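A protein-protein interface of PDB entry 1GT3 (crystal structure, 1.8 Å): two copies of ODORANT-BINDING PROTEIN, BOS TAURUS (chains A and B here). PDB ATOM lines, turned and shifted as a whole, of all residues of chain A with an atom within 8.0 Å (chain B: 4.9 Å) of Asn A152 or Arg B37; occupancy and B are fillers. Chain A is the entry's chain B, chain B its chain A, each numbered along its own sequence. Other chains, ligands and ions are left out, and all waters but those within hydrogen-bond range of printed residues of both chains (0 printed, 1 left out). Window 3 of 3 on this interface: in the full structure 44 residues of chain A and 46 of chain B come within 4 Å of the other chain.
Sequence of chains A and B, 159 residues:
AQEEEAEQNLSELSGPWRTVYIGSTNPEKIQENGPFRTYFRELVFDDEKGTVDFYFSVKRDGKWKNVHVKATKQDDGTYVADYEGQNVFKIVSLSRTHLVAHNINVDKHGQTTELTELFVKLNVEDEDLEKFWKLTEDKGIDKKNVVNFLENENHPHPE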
ATOM      1  N   ARG A  18      14.384   8.258 -30.329  1.00  0.00           N
ATOM      2  CA  ARG A  18      13.218   8.449 -29.471  1.00  0.00           C
ATOM      3  C   ARG A  18      12.044   7.567 -29.882  1.00  0.00           C
ATOM      4  O   ARG A  18      11.832   7.302 -31.061  1.00  0.00           O
ATOM      5  CB  ARG A  18      12.778   9.920 -29.505  1.00  0.00           C
ATOM      6  CG  ARG A  18      13.750  10.871 -28.841  1.00  0.00           C
ATOM      7  CD  ARG A  18      13.987  10.805 -27.347  1.00  0.00           C
ATOM      8  NE  ARG A  18      14.968  11.786 -26.889  1.00  0.00           N
ATOM      9  CZ  ARG A  18      16.273  11.554 -26.762  1.00  0.00           C
ATOM     10  NH1 ARG A  18      17.073  12.523 -26.337  1.00  0.00           N
ATOM     11  NH2 ARG A  18      16.775  10.359 -27.040  1.00  0.00           N
ATOM     12  N   ARG A  41      16.555   6.171 -25.554  1.00  0.00           N
ATOM     13  CA  ARG A  41      17.548   7.223 -25.330  1.00  0.00           C
ATOM     14  C   ARG A  41      18.571   7.197 -26.470  1.00  0.00           C
ATOM     15  O   ARG A  41      18.779   8.193 -27.159  1.00  0.00           O
ATOM     16  CB  ARG A  41      18.293   6.981 -24.016  1.00  0.00           C
ATOM     17  CG  ARG A  41      17.445   7.061 -22.757  1.00  0.00           C
ATOM     18  CD  ARG A  41      17.908   6.161 -21.555  1.00  0.00           C
ATOM     19  NE  ARG A  41      19.348   6.277 -21.314  1.00  0.00           N
ATOM     20  CZ  ARG A  41      20.082   5.341 -20.724  1.00  0.00           C
ATOM     21  NH1 ARG A  41      21.381   5.534 -20.547  1.00  0.00           N
ATOM     22  NH2 ARG A  41      19.524   4.206 -20.314  1.00  0.00           N
ATOM     23  N   ASN A  66      17.020   3.122 -15.717  1.00  0.00           N
ATOM     24  CA  ASN A  66      17.764   3.193 -16.971  1.00  0.00           C
ATOM     25  C   ASN A  66      18.209   1.759 -17.268  1.00  0.00           C
ATOM     26  O   ASN A  66      18.844   1.111 -16.432  1.00  0.00           O
ATOM     27  CB  ASN A  66      18.977   4.115 -16.847  1.00  0.00           C
ATOM     28  CG  ASN A  66      18.587   5.579 -16.722  1.00  0.00           C
ATOM     29  OD1 ASN A  66      17.583   6.016 -17.289  1.00  0.00           O
ATOM     30  ND2 ASN A  66      19.391   6.346 -15.994  1.00  0.00           N
ATOM     31  N   VAL A 146      27.623  27.078 -21.436  1.00  0.00           N
ATOM     32  CA  VAL A 146      26.738  26.423 -22.386  1.00  0.00           C
ATOM     33  C   VAL A 146      26.374  25.046 -21.843  1.00  0.00           C
ATOM     34  O   VAL A 146      27.245  24.282 -21.424  1.00  0.00           O
ATOM     35  CB  VAL A 146      27.414  26.261 -23.765  1.00  0.00           C
ATOM     36  CG1 VAL A 146      26.477  25.532 -24.722  1.00  0.00           C
ATOM     37  CG2 VAL A 146      27.797  27.635 -24.318  1.00  0.00           C
ATOM     38  N   VAL A 147      25.084  24.739 -21.847  1.00  0.00           N
ATOM     39  CA  VAL A 147      24.588  23.462 -21.356  1.00  0.00           C
ATOM     40  C   VAL A 147      24.139  22.560 -22.503  1.00  0.00           C
ATOM     41  O   VAL A 147      23.510  23.014 -23.458  1.00  0.00           O
ATOM     42  CB  VAL A 147      23.390  23.667 -20.401  1.00  0.00           C
ATOM     43  CG1 VAL A 147      22.750  22.322 -20.058  1.00  0.00           C
ATOM     44  CG2 VAL A 147      23.850  24.369 -19.137  1.00  0.00           C
ATOM     45  N   ASN A 148      24.467  21.276 -22.393  1.00  0.00           N
ATOM     46  CA  ASN A 148      24.092  20.288 -23.395  1.00  0.00           C
ATOM     47  C   ASN A 148      22.858  19.577 -22.850  1.00  0.00           C
ATOM     48  O   ASN A 148      22.966  18.690 -22.001  1.00  0.00           O
ATOM     49  CB  ASN A 148      25.240  19.287 -23.604  1.00  0.00           C
ATOM     50  CG  ASN A 148      25.022  18.374 -24.809  1.00  0.00           C
ATOM     51  OD1 ASN A 148      25.974  18.011 -25.509  1.00  0.00           O
ATOM     52  ND2 ASN A 148      23.778  17.992 -25.050  1.00  0.00           N
ATOM     53  N   PHE A 149      21.682  19.980 -23.330  1.00  0.00           N
ATOM     54  CA  PHE A 149      20.428  19.389 -22.880  1.00  0.00           C
ATOM     55  C   PHE A 149      20.203  17.994 -23.450  1.00  0.00           C
ATOM     56  O   PHE A 149      19.594  17.150 -22.803  1.00  0.00           O
ATOM     57  CB  PHE A 149      19.239  20.288 -23.258  1.00  0.00           C
ATOM     58  CG  PHE A 149      19.204  21.586 -22.506  1.00  0.00           C
ATOM     59  CD1 PHE A 149      20.155  22.573 -22.745  1.00  0.00           C
ATOM     60  CD2 PHE A 149      18.244  21.804 -21.518  1.00  0.00           C
ATOM     61  CE1 PHE A 149      20.158  23.756 -22.010  1.00  0.00           C
ATOM     62  CE2 PHE A 149      18.241  22.986 -20.775  1.00  0.00           C
ATOM     63  CZ  PHE A 149      19.198  23.959 -21.018  1.00  0.00           C
ATOM     64  N   LEU A 150      20.702  17.760 -24.658  1.00  0.00           N
ATOM     65  CA  LEU A 150      20.526  16.471 -25.314  1.00  0.00           C
ATOM     66  C   LEU A 150      21.169  15.321 -24.547  1.00  0.00           C
ATOM     67  O   LEU A 150      20.575  14.245 -24.420  1.00  0.00           O
ATOM     68  CB  LEU A 150      21.072  16.528 -26.746  1.00  0.00           C
ATOM     69  CG  LEU A 150      20.977  15.242 -27.573  1.00  0.00           C
ATOM     70  CD1 LEU A 150      19.529  14.793 -27.671  1.00  0.00           C
ATOM     71  CD2 LEU A 150      21.553  15.485 -28.961  1.00  0.00           C
ATOM     72  N   GLU A 151      22.378  15.532 -24.031  1.00  0.00           N
ATOM     73  CA  GLU A 151      23.040  14.471 -23.280  1.00  0.00           C
ATOM     74  C   GLU A 151      22.383  14.282 -21.914  1.00  0.00           C
ATOM     75  O   GLU A 151      22.493  13.212 -21.305  1.00  0.00           O
ATOM     76  CB  GLU A 151      24.540  14.757 -23.130  1.00  0.00           C
ATOM     77  CG  GLU A 151      25.291  14.771 -24.487  1.00  0.00           C
ATOM     78  CD  GLU A 151      25.085  13.498 -25.288  1.00  0.00           C
ATOM     79  OE1 GLU A 151      25.279  13.534 -26.522  1.00  0.00           O
ATOM     80  OE2 GLU A 151      24.738  12.453 -24.691  1.00  0.00           O
ATOM     81  N   ASN A 152      21.703  15.316 -21.428  1.00  0.00           N
ATOM     82  CA  ASN A 152      21.007  15.190 -20.149  1.00  0.00           C
ATOM     83  C   ASN A 152      19.829  14.242 -20.363  1.00  0.00           C
ATOM     84  O   ASN A 152      19.623  13.304 -19.589  1.00  0.00           O
ATOM     85  CB  ASN A 152      20.500  16.548 -19.658  1.00  0.00           C
ATOM     86  CG  ASN A 152      21.595  17.391 -19.042  1.00  0.00           C
ATOM     87  OD1 ASN A 152      22.700  16.908 -18.795  1.00  0.00           O
ATOM     88  ND2 ASN A 152      21.290  18.658 -18.773  1.00  0.00           N
ATOM     89  N   GLU A 153      19.064  14.484 -21.427  1.00  0.00           N
ATOM     90  CA  GLU A 153      17.927  13.630 -21.745  1.00  0.00           C
ATOM     91  C   GLU A 153      18.366  12.208 -22.094  1.00  0.00           C
ATOM     92  O   GLU A 153      17.629  11.264 -21.838  1.00  0.00           O
ATOM     93  CB  GLU A 153      17.115  14.205 -22.909  1.00  0.00           C
ATOM     94  CG  GLU A 153      16.330  15.494 -22.573  1.00  0.00           C
ATOM     95  CD  GLU A 153      15.271  15.802 -23.623  1.00  0.00           C
ATOM     96  OE1 GLU A 153      14.668  16.890 -23.582  1.00  0.00           O
ATOM     97  OE2 GLU A 153      15.040  14.943 -24.492  1.00  0.00           O
ATOM     98  N   ASN A 154      19.559  12.053 -22.674  1.00  0.00           N
ATOM     99  CA  ASN A 154      20.076  10.728 -23.047  1.00  0.00           C
ATOM    100  C   ASN A 154      20.591   9.953 -21.844  1.00  0.00           C
ATOM    101  O   ASN A 154      20.827   8.739 -21.920  1.00  0.00           O
ATOM    102  CB  ASN A 154      21.208  10.848 -24.080  1.00  0.00           C
ATOM    103  CG  ASN A 154      20.691  11.065 -25.496  1.00  0.00           C
ATOM    104  OD1 ASN A 154      21.470  11.171 -26.444  1.00  0.00           O
ATOM    105  ND2 ASN A 154      19.377  11.131 -25.640  1.00  0.00           N
ATOM    106  N   HIS A 155      20.781  10.659 -20.736  1.00  0.00           N
ATOM    107  CA  HIS A 155      21.263  10.037 -19.510  1.00  0.00           C
ATOM    108  C   HIS A 155      20.468  10.570 -18.323  1.00  0.00           C
ATOM    109  O   HIS A 155      21.010  11.291 -17.491  1.00  0.00           O
ATOM    110  CB  HIS A 155      22.743  10.348 -19.284  1.00  0.00           C
ATOM    111  CG  HIS A 155      23.616  10.059 -20.465  1.00  0.00           C
ATOM    112  ND1 HIS A 155      23.708  10.905 -21.548  1.00  0.00           N
ATOM    113  CD2 HIS A 155      24.444   9.020 -20.728  1.00  0.00           C
ATOM    114  CE1 HIS A 155      24.557  10.402 -22.425  1.00  0.00           C
ATOM    115  NE2 HIS A 155      25.017   9.257 -21.951  1.00  0.00           N
ATOM    116  N   PRO A 156      19.174  10.216 -18.229  1.00  0.00           N
ATOM    117  CA  PRO A 156      18.306  10.670 -17.135  1.00  0.00           C
ATOM    118  C   PRO A 156      18.549   9.946 -15.817  1.00  0.00           C
ATOM    119  O   PRO A 156      19.487   9.161 -15.690  1.00  0.00           O
ATOM    120  CB  PRO A 156      16.912  10.395 -17.681  1.00  0.00           C
ATOM    121  CG  PRO A 156      17.118   9.115 -18.424  1.00  0.00           C
ATOM    122  CD  PRO A 156      18.419   9.373 -19.173  1.00  0.00           C
ATOM    123  N   HIS A 157      17.694  10.215 -14.833  1.00  0.00           N
ATOM    124  CA  HIS A 157      17.822   9.572 -13.531  1.00  0.00           C
ATOM    125  C   HIS A 157      16.498   9.543 -12.779  1.00  0.00           C
ATOM    126  O   HIS A 157      15.489  10.028 -13.336  1.00  0.00           O
ATOM    127  CB  HIS A 157      18.885  10.284 -12.686  1.00  0.00           C
ATOM    128  CG  HIS A 157      18.495  11.663 -12.249  1.00  0.00           C
ATOM    129  ND1 HIS A 157      17.367  11.915 -11.497  1.00  0.00           N
ATOM    130  CD2 HIS A 157      19.098  12.861 -12.436  1.00  0.00           C
ATOM    131  CE1 HIS A 157      17.293  13.208 -11.239  1.00  0.00           C
ATOM    132  NE2 HIS A 157      18.331  13.804 -11.796  1.00  0.00           N
ATOM    133  N   LYS B  29      21.292  31.901 -14.968  1.00  0.00           N
ATOM    134  CA  LYS B  29      20.013  31.722 -15.656  1.00  0.00           C
ATOM    135  C   LYS B  29      19.795  30.321 -16.229  1.00  0.00           C
ATOM    136  O   LYS B  29      18.654  29.893 -16.404  1.00  0.00           O
ATOM    137  CB  LYS B  29      19.876  32.753 -16.780  1.00  0.00           C
ATOM    138  CG  LYS B  29      19.865  34.193 -16.293  1.00  0.00           C
ATOM    139  CD  LYS B  29      18.747  34.679 -15.375  1.00  0.00           C
ATOM    140  CE  LYS B  29      18.738  36.126 -14.883  1.00  0.00           C
ATOM    141  NZ  LYS B  29      17.459  36.461 -14.215  1.00  0.00           N
ATOM    142  N   ILE B  30      20.877  29.603 -16.521  1.00  0.00           N
ATOM    143  CA  ILE B  30      20.733  28.263 -17.086  1.00  0.00           C
ATOM    144  C   ILE B  30      21.265  27.131 -16.209  1.00  0.00           C
ATOM    145  O   ILE B  30      21.178  25.956 -16.577  1.00  0.00           O
ATOM    146  CB  ILE B  30      21.378  28.178 -18.490  1.00  0.00           C
ATOM    147  CG1 ILE B  30      22.865  28.518 -18.421  1.00  0.00           C
ATOM    148  CG2 ILE B  30      20.663  29.134 -19.435  1.00  0.00           C
ATOM    149  CD1 ILE B  30      23.592  28.350 -19.739  1.00  0.00           C
ATOM    150  N   GLN B  31      21.820  27.477 -15.051  1.00  0.00           N
ATOM    151  CA  GLN B  31      22.314  26.461 -14.126  1.00  0.00           C
ATOM    152  C   GLN B  31      21.089  25.771 -13.532  1.00  0.00           C
ATOM    153  O   GLN B  31      19.965  26.252 -13.685  1.00  0.00           O
ATOM    154  CB  GLN B  31      23.129  27.103 -13.000  1.00  0.00           C
ATOM    155  CG  GLN B  31      24.512  27.619 -13.421  1.00  0.00           C
ATOM    156  CD  GLN B  31      25.182  28.453 -12.340  1.00  0.00           C
ATOM    157  OE1 GLN B  31      26.324  28.882 -12.493  1.00  0.00           O
ATOM    158  NE2 GLN B  31      24.469  28.690 -11.243  1.00  0.00           N
ATOM    159  N   GLU B  32      21.300  24.650 -12.852  1.00  0.00           N
ATOM    160  CA  GLU B  32      20.184  23.940 -12.249  1.00  0.00           C
ATOM    161  C   GLU B  32      19.299  24.919 -11.483  1.00  0.00           C
ATOM    162  O   GLU B  32      19.793  25.783 -10.757  1.00  0.00           O
ATOM    163  CB  GLU B  32      20.697  22.840 -11.317  1.00  0.00           C
ATOM    164  CG  GLU B  32      21.705  21.923 -11.991  1.00  0.00           C
ATOM    165  CD  GLU B  32      21.502  20.468 -11.642  1.00  0.00           C
ATOM    166  OE1 GLU B  32      22.278  19.633 -12.151  1.00  0.00           O
ATOM    167  OE2 GLU B  32      20.570  20.160 -10.870  1.00  0.00           O
ATOM    168  N   ASN B  33      17.991  24.783 -11.679  1.00  0.00           N
ATOM    169  CA  ASN B  33      16.992  25.631 -11.045  1.00  0.00           C
ATOM    170  C   ASN B  33      16.890  26.998 -11.723  1.00  0.00           C
ATOM    171  O   ASN B  33      16.153  27.869 -11.267  1.00  0.00           O
ATOM    172  CB  ASN B  33      17.307  25.819  -9.558  1.00  0.00           C
ATOM    173  CG  ASN B  33      16.072  25.699  -8.683  1.00  0.00           C
ATOM    174  OD1 ASN B  33      15.985  26.329  -7.629  1.00  0.00           O
ATOM    175  ND2 ASN B  33      15.120  24.876  -9.109  1.00  0.00           N
ATOM    176  N   GLY B  34      17.628  27.183 -12.815  1.00  0.00           N
ATOM    177  CA  GLY B  34      17.586  28.449 -13.532  1.00  0.00           C
ATOM    178  C   GLY B  34      16.326  28.561 -14.373  1.00  0.00           C
ATOM    179  O   GLY B  34      15.819  27.545 -14.833  1.00  0.00           O
ATOM    180  N   PRO B  35      15.798  29.776 -14.604  1.00  0.00           N
ATOM    181  CA  PRO B  35      14.577  29.914 -15.405  1.00  0.00           C
ATOM    182  C   PRO B  35      14.710  29.581 -16.888  1.00  0.00           C
ATOM    183  O   PRO B  35      13.716  29.270 -17.547  1.00  0.00           O
ATOM    184  CB  PRO B  35      14.178  31.369 -15.174  1.00  0.00           C
ATOM    185  CG  PRO B  35      15.498  32.053 -15.038  1.00  0.00           C
ATOM    186  CD  PRO B  35      16.276  31.095 -14.149  1.00  0.00           C
ATOM    187  N   PHE B  36      15.923  29.645 -17.422  1.00  0.00           N
ATOM    188  CA  PHE B  36      16.093  29.342 -18.831  1.00  0.00           C
ATOM    189  C   PHE B  36      16.703  27.986 -19.138  1.00  0.00           C
ATOM    190  O   PHE B  36      17.197  27.764 -20.244  1.00  0.00           O
ATOM    191  CB  PHE B  36      16.875  30.453 -19.522  1.00  0.00           C
ATOM    192  CG  PHE B  36      16.074  31.709 -19.704  1.00  0.00           C
ATOM    193  CD1 PHE B  36      15.959  32.637 -18.672  1.00  0.00           C
ATOM    194  CD2 PHE B  36      15.358  31.918 -20.873  1.00  0.00           C
ATOM    195  CE1 PHE B  36      15.131  33.755 -18.806  1.00  0.00           C
ATOM    196  CE2 PHE B  36      14.529  33.025 -21.019  1.00  0.00           C
ATOM    197  CZ  PHE B  36      14.416  33.947 -19.983  1.00  0.00           C
ATOM    198  N   ARG B  37      16.671  27.090 -18.157  1.00  0.00           N
ATOM    199  CA  ARG B  37      17.166  25.722 -18.335  1.00  0.00           C
ATOM    200  C   ARG B  37      15.927  24.994 -18.835  1.00  0.00           C
ATOM    201  O   ARG B  37      15.378  24.116 -18.169  1.00  0.00           O
ATOM    202  CB  ARG B  37      17.619  25.145 -16.994  1.00  0.00           C
ATOM    203  CG  ARG B  37      18.031  23.689 -17.049  1.00  0.00           C
ATOM    204  CD  ARG B  37      18.780  23.094 -15.880  1.00  0.00           C
ATOM    205  NE  ARG B  37      20.147  23.589 -15.867  1.00  0.00           N
ATOM    206  CZ  ARG B  37      21.221  22.826 -16.038  1.00  0.00           C
ATOM    207  NH1 ARG B  37      21.097  21.521 -16.221  1.00  0.00           N
ATOM    208  NH2 ARG B  37      22.422  23.382 -16.048  1.00  0.00           N
ATOM    209  N   THR B  38      15.506  25.376 -20.035  1.00  0.00           N
ATOM    210  CA  THR B  38      14.284  24.874 -20.638  1.00  0.00           C
ATOM    211  C   THR B  38      14.380  23.716 -21.615  1.00  0.00           C
ATOM    212  O   THR B  38      15.088  23.793 -22.607  1.00  0.00           O
ATOM    213  CB  THR B  38      13.553  26.025 -21.352  1.00  0.00           C
ATOM    214  OG1 THR B  38      14.397  26.565 -22.377  1.00  0.00           O
ATOM    215  CG2 THR B  38      13.215  27.141 -20.359  1.00  0.00           C
ATOM    216  N   TYR B  39      13.643  22.649 -21.319  1.00  0.00           N
ATOM    217  CA  TYR B  39      13.593  21.476 -22.185  1.00  0.00           C
ATOM    218  C   TYR B  39      12.354  21.638 -23.069  1.00  0.00           C
ATOM    219  O   TYR B  39      11.223  21.457 -22.615  1.00  0.00           O
ATOM    220  CB  TYR B  39      13.484  20.193 -21.350  1.00  0.00           C
ATOM    221  CG  TYR B  39      14.739  19.851 -20.569  1.00  0.00           C
ATOM    222  CD1 TYR B  39      15.724  19.023 -21.122  1.00  0.00           C
ATOM    223  CD2 TYR B  39      14.960  20.369 -19.290  1.00  0.00           C
ATOM    224  CE1 TYR B  39      16.892  18.722 -20.422  1.00  0.00           C
ATOM    225  CE2 TYR B  39      16.137  20.073 -18.580  1.00  0.00           C
ATOM    226  CZ  TYR B  39      17.095  19.247 -19.161  1.00  0.00           C
ATOM    227  OH  TYR B  39      18.263  18.940 -18.499  1.00  0.00           O
ATOM    228  N   SER B  57       9.390  22.459 -20.565  1.00  0.00           N
ATOM    229  CA  SER B  57       9.389  22.068 -19.161  1.00  0.00           C
ATOM    230  C   SER B  57      10.625  22.621 -18.474  1.00  0.00           C
ATOM    231  O   SER B  57      11.698  22.691 -19.071  1.00  0.00           O
ATOM    232  CB  SER B  57       9.388  20.545 -19.030  1.00  0.00           C
ATOM    233  OG  SER B  57       8.257  19.981 -19.662  1.00  0.00           O
ATOM    234  N   VAL B  58      10.469  23.016 -17.217  1.00  0.00           N
ATOM    235  CA  VAL B  58      11.579  23.554 -16.448  1.00  0.00           C
ATOM    236  C   VAL B  58      11.406  23.107 -15.005  1.00  0.00           C
ATOM    237  O   VAL B  58      10.280  22.958 -14.525  1.00  0.00           O
ATOM    238  CB  VAL B  58      11.618  25.107 -16.498  1.00  0.00           C
ATOM    239  CG1 VAL B  58      10.596  25.696 -15.533  1.00  0.00           C
ATOM    240  CG2 VAL B  58      13.017  25.601 -16.166  1.00  0.00           C
ATOM    241  N   PRO B 158      14.988  14.505 -17.109  1.00  0.00           N
ATOM    242  CA  PRO B 158      16.383  14.685 -17.523  1.00  0.00           C
ATOM    243  C   PRO B 158      17.288  15.082 -16.361  1.00  0.00           C
ATOM    244  O   PRO B 158      18.512  15.051 -16.479  1.00  0.00           O
ATOM    245  CB  PRO B 158      16.283  15.776 -18.583  1.00  0.00           C
ATOM    246  CG  PRO B 158      15.123  16.596 -18.102  1.00  0.00           C
ATOM    247  CD  PRO B 158      14.125  15.545 -17.693  1.00  0.00           C
ATOM    248  N   GLU B 159      16.678  15.450 -15.239  1.00  0.00           N
ATOM    249  CA  GLU B 159      17.424  15.860 -14.055  1.00  0.00           C
ATOM    250  C   GLU B 159      16.513  15.991 -12.839  1.00  0.00           C
ATOM    251  O   GLU B 159      15.298  15.741 -12.984  1.00  0.00           O
ATOM    252  CB  GLU B 159      18.130  17.196 -14.316  1.00  0.00           C
ATOM    253  CG  GLU B 159      17.270  18.220 -15.050  1.00  0.00           C
ATOM    254  CD  GLU B 159      17.918  19.588 -15.119  1.00  0.00           C
ATOM    255  OE1 GLU B 159      17.871  20.323 -14.110  1.00  0.00           O
ATOM    256  OE2 GLU B 159      18.484  19.929 -16.176  1.00  0.00           O
ATOM    257  OXT GLU B 159      17.030  16.342 -11.757  1.00  0.00           O
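The side-chain hydroxyl (OH) of Tyr B39 is in hydrogen-bond range of the side-chain amide nitrogen (ND2) of Asn A152, 3.1 Å away. The chain-end carboxylate (OXT) of Glu B159 is in hydrogen-bond range of a ring nitrogen (NE2) of His A157, 2.9 Å away.
OH of Tyr B39 is in hydrogen-bond range of OE2 of Glu B159 (2.5 Å). The backbone carbonyl oxygen of Ile B30 sits at hydrogen-bond distance from the guanidinium group of Arg B37, 2.7 Å away. The backbone carbonyl oxygen of Tyr B39 is in hydrogen-bond range of the backbone NH of Ser B57. The guanidinium group (NH1) of Arg B37 lies within salt-bridge range of the side-chain carboxylate (OE2) of Glu B159, at 3.1 Å. OE2 of Glu A153 lies within salt-bridge range of NH1 of Arg A18, 3.7 Å away. O of Gln B31 lies close to NE of Arg B37, at 3.4 Å.
Arg B37 touches Val A147. Arg B37 touches Phe A149. Phe A149 touches Thr B38. Phe A149 touches Tyr B39. Arg B37 touches Asn A152. Asn A152 touches Pro B158 (O to O, 3.7 Å). Glu A153 touches Tyr B39.
Printed residues of chain B within 4 Å of Val A147: Arg B37. Of chain B, only Arg B37, Tyr B39 and Pro B158 come within 4 Å of Asn A152. Gly B34 touches none of the printed residues of chain A. Of chain A, only Val A147, Phe A149 and Asn A152 come within 4 Å of Arg B37. Of the printed residues of chain A, Tyr B39 touches Phe A149, Asn A152 and Glu A153. Printed residues of chain A within 4 Å of Glu B159: His A157. The nearest residue of chain A that does not touch Arg B37 is Asn A148 (6.7 Å). The nearest printed residue of chain B that does not touch Phe A149 is Phe B36 (4.4 Å).
Printed residues of chain B that touch a printed residue of chain A: Arg B37, Thr B38, Tyr B39, Pro B158 and Glu B159. Along chain B the printed residues that touch a printed residue of chain A span positions 37 to 159. Of the 15 printed residues of chain A, 5 touch a printed residue of chain B. Hydrophobic or aromatic side chains of chain A that line the printed part of chain B: Val A147, Phe A149 and His A157. Among the printed residues, no Asp or Glu carboxylate lies within 4 Å of a Lys or Arg side-chain nitrogen of the other chain.
No position is printed for both chains. Of the 9 pairs that touch across the chains among the printed residues, none has its exchanged pair printed and touching as well.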
